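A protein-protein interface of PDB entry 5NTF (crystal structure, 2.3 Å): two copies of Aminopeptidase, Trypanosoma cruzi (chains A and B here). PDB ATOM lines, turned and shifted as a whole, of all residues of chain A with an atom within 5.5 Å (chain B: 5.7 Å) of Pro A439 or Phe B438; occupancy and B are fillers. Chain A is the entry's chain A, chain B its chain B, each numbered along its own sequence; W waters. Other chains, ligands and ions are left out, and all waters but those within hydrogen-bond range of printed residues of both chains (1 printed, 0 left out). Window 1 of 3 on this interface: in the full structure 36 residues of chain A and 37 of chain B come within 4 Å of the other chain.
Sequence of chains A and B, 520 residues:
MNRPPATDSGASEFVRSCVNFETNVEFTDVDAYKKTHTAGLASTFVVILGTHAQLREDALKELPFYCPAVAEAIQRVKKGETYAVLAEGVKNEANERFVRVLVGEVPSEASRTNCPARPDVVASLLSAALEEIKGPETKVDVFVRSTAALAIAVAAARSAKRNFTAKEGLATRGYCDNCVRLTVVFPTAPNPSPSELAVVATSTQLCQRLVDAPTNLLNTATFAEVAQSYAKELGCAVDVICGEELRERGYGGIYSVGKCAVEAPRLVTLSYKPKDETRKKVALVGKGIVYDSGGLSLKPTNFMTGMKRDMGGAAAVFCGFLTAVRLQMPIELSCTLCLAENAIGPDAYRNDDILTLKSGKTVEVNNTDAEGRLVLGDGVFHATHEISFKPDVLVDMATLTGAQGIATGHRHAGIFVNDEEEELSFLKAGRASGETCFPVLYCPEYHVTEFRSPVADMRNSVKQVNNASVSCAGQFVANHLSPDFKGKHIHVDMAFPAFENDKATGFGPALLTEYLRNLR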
ATOM      1  N   THR A 408      -0.860  -6.817  17.632  1.00  0.00           N
ATOM      2  CA  THR A 408      -1.239  -6.293  16.313  1.00  0.00           C
ATOM      3  C   THR A 408      -2.697  -6.552  15.853  1.00  0.00           C
ATOM      4  O   THR A 408      -3.073  -6.214  14.729  1.00  0.00           O
ATOM      5  CB  THR A 408      -0.253  -6.779  15.228  1.00  0.00           C
ATOM      6  OG1 THR A 408      -0.362  -8.196  15.049  1.00  0.00           O
ATOM      7  CG2 THR A 408       1.186  -6.416  15.590  1.00  0.00           C
ATOM      8  N   ALA A 413      -1.258  -9.396  10.723  1.00  0.00           N
ATOM      9  CA  ALA A 413      -0.210 -10.315  11.119  1.00  0.00           C
ATOM     10  C   ALA A 413       0.988  -9.511  11.648  1.00  0.00           C
ATOM     11  O   ALA A 413       1.317  -8.459  11.107  1.00  0.00           O
ATOM     12  CB  ALA A 413       0.205 -11.200   9.951  1.00  0.00           C
ATOM     13  N   GLY A 414       1.589  -9.976  12.738  1.00  0.00           N
ATOM     14  CA  GLY A 414       2.754  -9.312  13.293  1.00  0.00           C
ATOM     15  C   GLY A 414       3.982  -9.761  12.532  1.00  0.00           C
ATOM     16  O   GLY A 414       4.139 -10.956  12.251  1.00  0.00           O
ATOM     17  N   ILE A 415       4.833  -8.803  12.179  1.00  0.00           N
ATOM     18  CA  ILE A 415       6.078  -9.132  11.478  1.00  0.00           C
ATOM     19  C   ILE A 415       7.359  -8.662  12.198  1.00  0.00           C
ATOM     20  O   ILE A 415       7.520  -7.500  12.568  1.00  0.00           O
ATOM     21  CB  ILE A 415       6.084  -8.704   9.994  1.00  0.00           C
ATOM     22  CG1 ILE A 415       5.920  -7.197   9.843  1.00  0.00           C
ATOM     23  CG2 ILE A 415       5.003  -9.475   9.250  1.00  0.00           C
ATOM     24  CD1 ILE A 415       5.976  -6.711   8.396  1.00  0.00           C
ATOM     25  N   GLU A 423      11.060  -4.924   5.334  1.00  0.00           N
ATOM     26  CA  GLU A 423       9.873  -4.812   6.161  1.00  0.00           C
ATOM     27  C   GLU A 423       8.865  -3.920   5.452  1.00  0.00           C
ATOM     28  O   GLU A 423       7.688  -4.262   5.367  1.00  0.00           O
ATOM     29  CB  GLU A 423      10.230  -4.241   7.542  1.00  0.00           C
ATOM     30  CG  GLU A 423       9.039  -3.847   8.400  1.00  0.00           C
ATOM     31  CD  GLU A 423       9.449  -3.444   9.812  1.00  0.00           C
ATOM     32  OE1 GLU A 423       9.539  -2.224  10.062  1.00  0.00           O
ATOM     33  OE2 GLU A 423       9.655  -4.349  10.667  1.00  0.00           O
ATOM     34  N   LEU A 427       5.251  -4.925   4.081  1.00  0.00           N
ATOM     35  CA  LEU A 427       4.033  -4.184   4.435  1.00  0.00           C
ATOM     36  C   LEU A 427       3.245  -3.681   3.194  1.00  0.00           C
ATOM     37  O   LEU A 427       2.019  -3.731   3.191  1.00  0.00           O
ATOM     38  CB  LEU A 427       4.356  -2.999   5.343  1.00  0.00           C
ATOM     39  CG  LEU A 427       4.885  -3.329   6.734  1.00  0.00           C
ATOM     40  CD1 LEU A 427       5.368  -2.066   7.452  1.00  0.00           C
ATOM     41  CD2 LEU A 427       3.805  -4.012   7.548  1.00  0.00           C
ATOM     42  N   CYS A 437      -0.287  -6.641   7.328  1.00  0.00           N
ATOM     43  CA  CYS A 437       0.646  -6.868   8.417  1.00  0.00           C
ATOM     44  C   CYS A 437       0.968  -5.574   9.166  1.00  0.00           C
ATOM     45  O   CYS A 437       0.634  -4.478   8.704  1.00  0.00           O
ATOM     46  CB  CYS A 437       1.930  -7.424   7.854  1.00  0.00           C
ATOM     47  SG  CYS A 437       1.712  -8.987   6.989  1.00  0.00           S
ATOM     48  N   PHE A 438       1.597  -5.723  10.338  1.00  0.00           N
ATOM     49  CA  PHE A 438       2.195  -4.591  11.096  1.00  0.00           C
ATOM     50  C   PHE A 438       3.457  -5.073  11.813  1.00  0.00           C
ATOM     51  O   PHE A 438       3.488  -6.191  12.305  1.00  0.00           O
ATOM     52  CB  PHE A 438       1.220  -3.975  12.086  1.00  0.00           C
ATOM     53  CG  PHE A 438       1.606  -2.583  12.529  1.00  0.00           C
ATOM     54  CD1 PHE A 438       1.371  -1.458  11.695  1.00  0.00           C
ATOM     55  CD2 PHE A 438       2.248  -2.376  13.735  1.00  0.00           C
ATOM     56  CE1 PHE A 438       1.748  -0.161  12.085  1.00  0.00           C
ATOM     57  CE2 PHE A 438       2.631  -1.080  14.127  1.00  0.00           C
ATOM     58  CZ  PHE A 438       2.385   0.029  13.309  1.00  0.00           C
ATOM     59  N   PRO A 439       4.507  -4.234  11.868  1.00  0.00           N
ATOM     60  CA  PRO A 439       5.721  -4.662  12.559  1.00  0.00           C
ATOM     61  C   PRO A 439       5.585  -4.853  14.049  1.00  0.00           C
ATOM     62  O   PRO A 439       4.904  -4.089  14.736  1.00  0.00           O
ATOM     63  CB  PRO A 439       6.718  -3.502  12.311  1.00  0.00           C
ATOM     64  CG  PRO A 439       6.125  -2.703  11.202  1.00  0.00           C
ATOM     65  CD  PRO A 439       4.644  -2.848  11.369  1.00  0.00           C
ATOM     66  N   VAL A 440       6.306  -5.845  14.542  1.00  0.00           N
ATOM     67  CA  VAL A 440       6.642  -5.901  15.961  1.00  0.00           C
ATOM     68  C   VAL A 440       8.101  -5.502  16.158  1.00  0.00           C
ATOM     69  O   VAL A 440       8.909  -5.511  15.224  1.00  0.00           O
ATOM     70  CB  VAL A 440       6.304  -7.252  16.603  1.00  0.00           C
ATOM     71  CG1 VAL A 440       4.823  -7.475  16.495  1.00  0.00           C
ATOM     72  CG2 VAL A 440       7.054  -8.411  15.971  1.00  0.00           C
ATOM     73  N   LEU A 441       8.406  -5.148  17.399  1.00  0.00           N
ATOM     74  CA  LEU A 441       9.743  -4.725  17.819  1.00  0.00           C
ATOM     75  C   LEU A 441      10.825  -5.664  17.334  1.00  0.00           C
ATOM     76  O   LEU A 441      10.789  -6.858  17.662  1.00  0.00           O
ATOM     77  CB  LEU A 441       9.814  -4.665  19.346  1.00  0.00           C
ATOM     78  CG  LEU A 441      11.158  -4.211  19.935  1.00  0.00           C
ATOM     79  CD1 LEU A 441      11.508  -2.800  19.466  1.00  0.00           C
ATOM     80  CD2 LEU A 441      11.139  -4.260  21.461  1.00  0.00           C
ATOM     81  N   TYR A 442      11.776  -5.123  16.574  1.00  0.00           N
ATOM     82  CA  TYR A 442      13.034  -5.828  16.280  1.00  0.00           C
ATOM     83  C   TYR A 442      14.150  -5.237  17.142  1.00  0.00           C
ATOM     84  O   TYR A 442      14.576  -4.086  16.946  1.00  0.00           O
ATOM     85  CB  TYR A 442      13.442  -5.779  14.804  1.00  0.00           C
ATOM     86  CG  TYR A 442      14.639  -6.691  14.495  1.00  0.00           C
ATOM     87  CD1 TYR A 442      14.474  -8.055  14.328  1.00  0.00           C
ATOM     88  CD2 TYR A 442      15.927  -6.173  14.375  1.00  0.00           C
ATOM     89  CE1 TYR A 442      15.531  -8.871  14.050  1.00  0.00           C
ATOM     90  CE2 TYR A 442      17.014  -6.984  14.092  1.00  0.00           C
ATOM     91  CZ  TYR A 442      16.809  -8.331  13.933  1.00  0.00           C
ATOM     92  OH  TYR A 442      17.888  -9.157  13.691  1.00  0.00           O
ATOM     93  N   THR B 113      16.139  -0.154  16.078  1.00  0.00           N
ATOM     94  CA  THR B 113      15.136   0.379  17.021  1.00  0.00           C
ATOM     95  C   THR B 113      15.708   0.840  18.367  1.00  0.00           C
ATOM     96  O   THR B 113      14.954   1.206  19.246  1.00  0.00           O
ATOM     97  CB  THR B 113      14.092  -0.685  17.364  1.00  0.00           C
ATOM     98  OG1 THR B 113      14.706  -1.715  18.142  1.00  0.00           O
ATOM     99  CG2 THR B 113      13.498  -1.283  16.088  1.00  0.00           C
ATOM    100  N   THR B 408       5.242  -4.094  23.154  1.00  0.00           N
ATOM    101  CA  THR B 408       6.521  -3.428  22.865  1.00  0.00           C
ATOM    102  C   THR B 408       7.634  -3.592  23.931  1.00  0.00           C
ATOM    103  O   THR B 408       8.721  -3.036  23.782  1.00  0.00           O
ATOM    104  CB  THR B 408       6.315  -1.931  22.557  1.00  0.00           C
ATOM    105  OG1 THR B 408       5.876  -1.245  23.723  1.00  0.00           O
ATOM    106  CG2 THR B 408       5.306  -1.726  21.415  1.00  0.00           C
ATOM    107  N   HIS B 412      10.741  -0.177  25.450  1.00  0.00           N
ATOM    108  CA  HIS B 412      10.187   0.618  24.365  1.00  0.00           C
ATOM    109  C   HIS B 412       8.744   0.993  24.636  1.00  0.00           C
ATOM    110  O   HIS B 412       7.868   0.128  24.666  1.00  0.00           O
ATOM    111  CB  HIS B 412      10.252  -0.128  23.054  1.00  0.00           C
ATOM    112  CG  HIS B 412      11.630  -0.337  22.535  1.00  0.00           C
ATOM    113  ND1 HIS B 412      12.422  -1.386  22.933  1.00  0.00           N
ATOM    114  CD2 HIS B 412      12.347   0.345  21.613  1.00  0.00           C
ATOM    115  CE1 HIS B 412      13.575  -1.334  22.289  1.00  0.00           C
ATOM    116  NE2 HIS B 412      13.548  -0.298  21.474  1.00  0.00           N
ATOM    117  N   ALA B 413       8.520   2.281  24.851  1.00  0.00           N
ATOM    118  CA  ALA B 413       7.196   2.821  25.004  1.00  0.00           C
ATOM    119  C   ALA B 413       6.466   2.608  23.701  1.00  0.00           C
ATOM    120  O   ALA B 413       7.036   2.765  22.625  1.00  0.00           O
ATOM    121  CB  ALA B 413       7.237   4.309  25.379  1.00  0.00           C
ATOM    122  N   GLY B 414       5.213   2.204  23.788  1.00  0.00           N
ATOM    123  CA  GLY B 414       4.399   2.019  22.599  1.00  0.00           C
ATOM    124  C   GLY B 414       3.867   3.361  22.159  1.00  0.00           C
ATOM    125  O   GLY B 414       3.387   4.149  22.985  1.00  0.00           O
ATOM    126  N   ILE B 415       3.945   3.633  20.862  1.00  0.00           N
ATOM    127  CA  ILE B 415       3.388   4.883  20.324  1.00  0.00           C
ATOM    128  C   ILE B 415       2.332   4.679  19.239  1.00  0.00           C
ATOM    129  O   ILE B 415       2.512   3.972  18.244  1.00  0.00           O
ATOM    130  CB  ILE B 415       4.460   5.883  19.865  1.00  0.00           C
ATOM    131  CG1 ILE B 415       5.330   5.299  18.748  1.00  0.00           C
ATOM    132  CG2 ILE B 415       5.293   6.298  21.065  1.00  0.00           C
ATOM    133  CD1 ILE B 415       6.378   6.277  18.212  1.00  0.00           C
ATOM    134  N   LEU B 427      10.221   8.638  16.950  1.00  0.00           N
ATOM    135  CA  LEU B 427      11.164   7.515  17.101  1.00  0.00           C
ATOM    136  C   LEU B 427      12.653   7.936  17.092  1.00  0.00           C
ATOM    137  O   LEU B 427      13.448   7.404  17.872  1.00  0.00           O
ATOM    138  CB  LEU B 427      10.957   6.444  16.010  1.00  0.00           C
ATOM    139  CG  LEU B 427       9.633   5.695  16.064  1.00  0.00           C
ATOM    140  CD1 LEU B 427       9.428   4.819  14.834  1.00  0.00           C
ATOM    141  CD2 LEU B 427       9.541   4.852  17.332  1.00  0.00           C
ATOM    142  N   THR B 436      13.711   4.994  24.388  1.00  0.00           N
ATOM    143  CA  THR B 436      13.259   4.481  23.090  1.00  0.00           C
ATOM    144  C   THR B 436      11.766   4.111  23.045  1.00  0.00           C
ATOM    145  O   THR B 436      11.159   3.692  24.056  1.00  0.00           O
ATOM    146  CB  THR B 436      14.067   3.245  22.698  1.00  0.00           C
ATOM    147  OG1 THR B 436      14.072   2.317  23.795  1.00  0.00           O
ATOM    148  CG2 THR B 436      15.461   3.631  22.380  1.00  0.00           C
ATOM    149  N   CYS B 437      11.205   4.277  21.854  1.00  0.00           N
ATOM    150  CA  CYS B 437       9.811   3.928  21.563  1.00  0.00           C
ATOM    151  C   CYS B 437       9.719   2.937  20.412  1.00  0.00           C
ATOM    152  O   CYS B 437      10.693   2.686  19.717  1.00  0.00           O
ATOM    153  CB  CYS B 437       9.063   5.178  21.186  1.00  0.00           C
ATOM    154  SG  CYS B 437       9.032   6.427  22.488  1.00  0.00           S
ATOM    155  N   PHE B 438       8.521   2.383  20.224  1.00  0.00           N
ATOM    156  CA  PHE B 438       8.177   1.593  19.013  1.00  0.00           C
ATOM    157  C   PHE B 438       6.711   1.758  18.684  1.00  0.00           C
ATOM    158  O   PHE B 438       5.881   1.827  19.605  1.00  0.00           O
ATOM    159  CB  PHE B 438       8.490   0.102  19.188  1.00  0.00           C
ATOM    160  CG  PHE B 438       8.589  -0.644  17.889  1.00  0.00           C
ATOM    161  CD1 PHE B 438       9.742  -0.565  17.101  1.00  0.00           C
ATOM    162  CD2 PHE B 438       7.533  -1.420  17.448  1.00  0.00           C
ATOM    163  CE1 PHE B 438       9.829  -1.272  15.892  1.00  0.00           C
ATOM    164  CE2 PHE B 438       7.623  -2.120  16.250  1.00  0.00           C
ATOM    165  CZ  PHE B 438       8.770  -2.031  15.460  1.00  0.00           C
ATOM    166  N   PRO B 439       6.362   1.814  17.377  1.00  0.00           N
ATOM    167  CA  PRO B 439       4.959   2.003  17.043  1.00  0.00           C
ATOM    168  C   PRO B 439       4.036   0.828  17.367  1.00  0.00           C
ATOM    169  O   PRO B 439       4.401  -0.338  17.247  1.00  0.00           O
ATOM    170  CB  PRO B 439       4.975   2.176  15.523  1.00  0.00           C
ATOM    171  CG  PRO B 439       6.387   2.444  15.161  1.00  0.00           C
ATOM    172  CD  PRO B 439       7.182   1.702  16.170  1.00  0.00           C
ATOM    173  N   VAL B 440       2.832   1.173  17.752  1.00  0.00           N
ATOM    174  CA  VAL B 440       1.736   0.225  17.710  1.00  0.00           C
ATOM    175  C   VAL B 440       0.834   0.557  16.526  1.00  0.00           C
ATOM    176  O   VAL B 440       0.865   1.684  15.992  1.00  0.00           O
ATOM    177  CB  VAL B 440       0.958   0.126  19.041  1.00  0.00           C
ATOM    178  CG1 VAL B 440       1.915  -0.360  20.114  1.00  0.00           C
ATOM    179  CG2 VAL B 440       0.325   1.454  19.448  1.00  0.00           C
HETATM  180  O   HOH W   1       4.008  -2.975  17.087  1.00  0.00           O
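Hydrophobic or aromatic side chains of chain A within 4 Å of the printed part of chain B: Phe A438 and Leu A441. Of the 12 printed residues of chain B, 6 touch a printed residue of chain A. Printed residues of chain B that touch a printed residue of chain A: Thr B113, Thr B408, His B412, Phe B438, Pro B439 and Val B440. Hydrophobic or aromatic side chains of chain B within 4 Å of the printed part of chain A: His B412 and Phe B438. Among the printed residues, no Asp or Glu carboxylate lies within 4 Å of a Lys or Arg side-chain nitrogen of the other chain.
The backbone carbonyl oxygen (O) of Tyr A442 is in hydrogen-bond range of the side-chain hydroxyl (OG1) of Thr B113 (2.7 Å).
Of the printed residues of chain B, Pro A439 touches Phe B438. Phe B438 touches just these residues of chain A: Pro A439 (3.7 Å), Val A440 (3.4 Å) and Leu A441 (3.3 Å). Of the printed residues of chain A, Pro B439 touches Phe A438. Printed residues of chain A within 4 Å of His B412: Leu A441. Printed residues of chain B within 4 Å of Leu A441: Thr B113, Thr B408, His B412 and Phe B438. Ile A415 touches none of the printed residues of chain B. Ile B415 touches none of the printed residues of chain A. The nearest residue of chain A that does not touch Phe B438 is Tyr A442 (4.4 Å).
Phe A438 touches Pro B439, and with the chains exchanged Pro A439 touches Phe B438. Phe A438 touches Val B440, and with the chains exchanged Val A440 touches Phe B438. Of the 9 pairs that touch across the chains among the printed residues, 4 have their exchanged pair printed and touching as well.
O of Ile A415 sits at hydrogen-bond distance from N of Val A440 (2.8 Å). N of Phe B438 sits at hydrogen-bond distance from O of Ala B413 (2.8 Å). The backbone carbonyl oxygen of Thr B113 is in hydrogen-bond range of a ring nitrogen (NE2) of His B412 (3.0 Å). N of Ile A415 lies within hydrogen-bond range of O of Phe A438, 2.9 Å away. N of Ile B415 lies within hydrogen-bond range of O of Phe B438. OG1 of Thr B408 sits at hydrogen-bond distance from O of His B412, 2.6 Å away.
Among the printed residues, pairs that only touch across the chains: Leu A441 with Phe B438 (3.3 Å), Phe A438 with Val B440 (3.4 Å), Val A440 with Phe B438 (3.4 Å), Leu A441 with His B412 (3.5 Å), Leu A441 with Thr B408 (3.6 Å), Leu A441 with Thr B113 (3.6 Å), Phe A438 with Pro B439 (3.7 Å) and Pro A439 with Phe B438 (3.7 Å).
Water W1 bridges the backbone carbonyl oxygen of Pro B439 and the backbone carbonyl oxygen of Pro A439.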
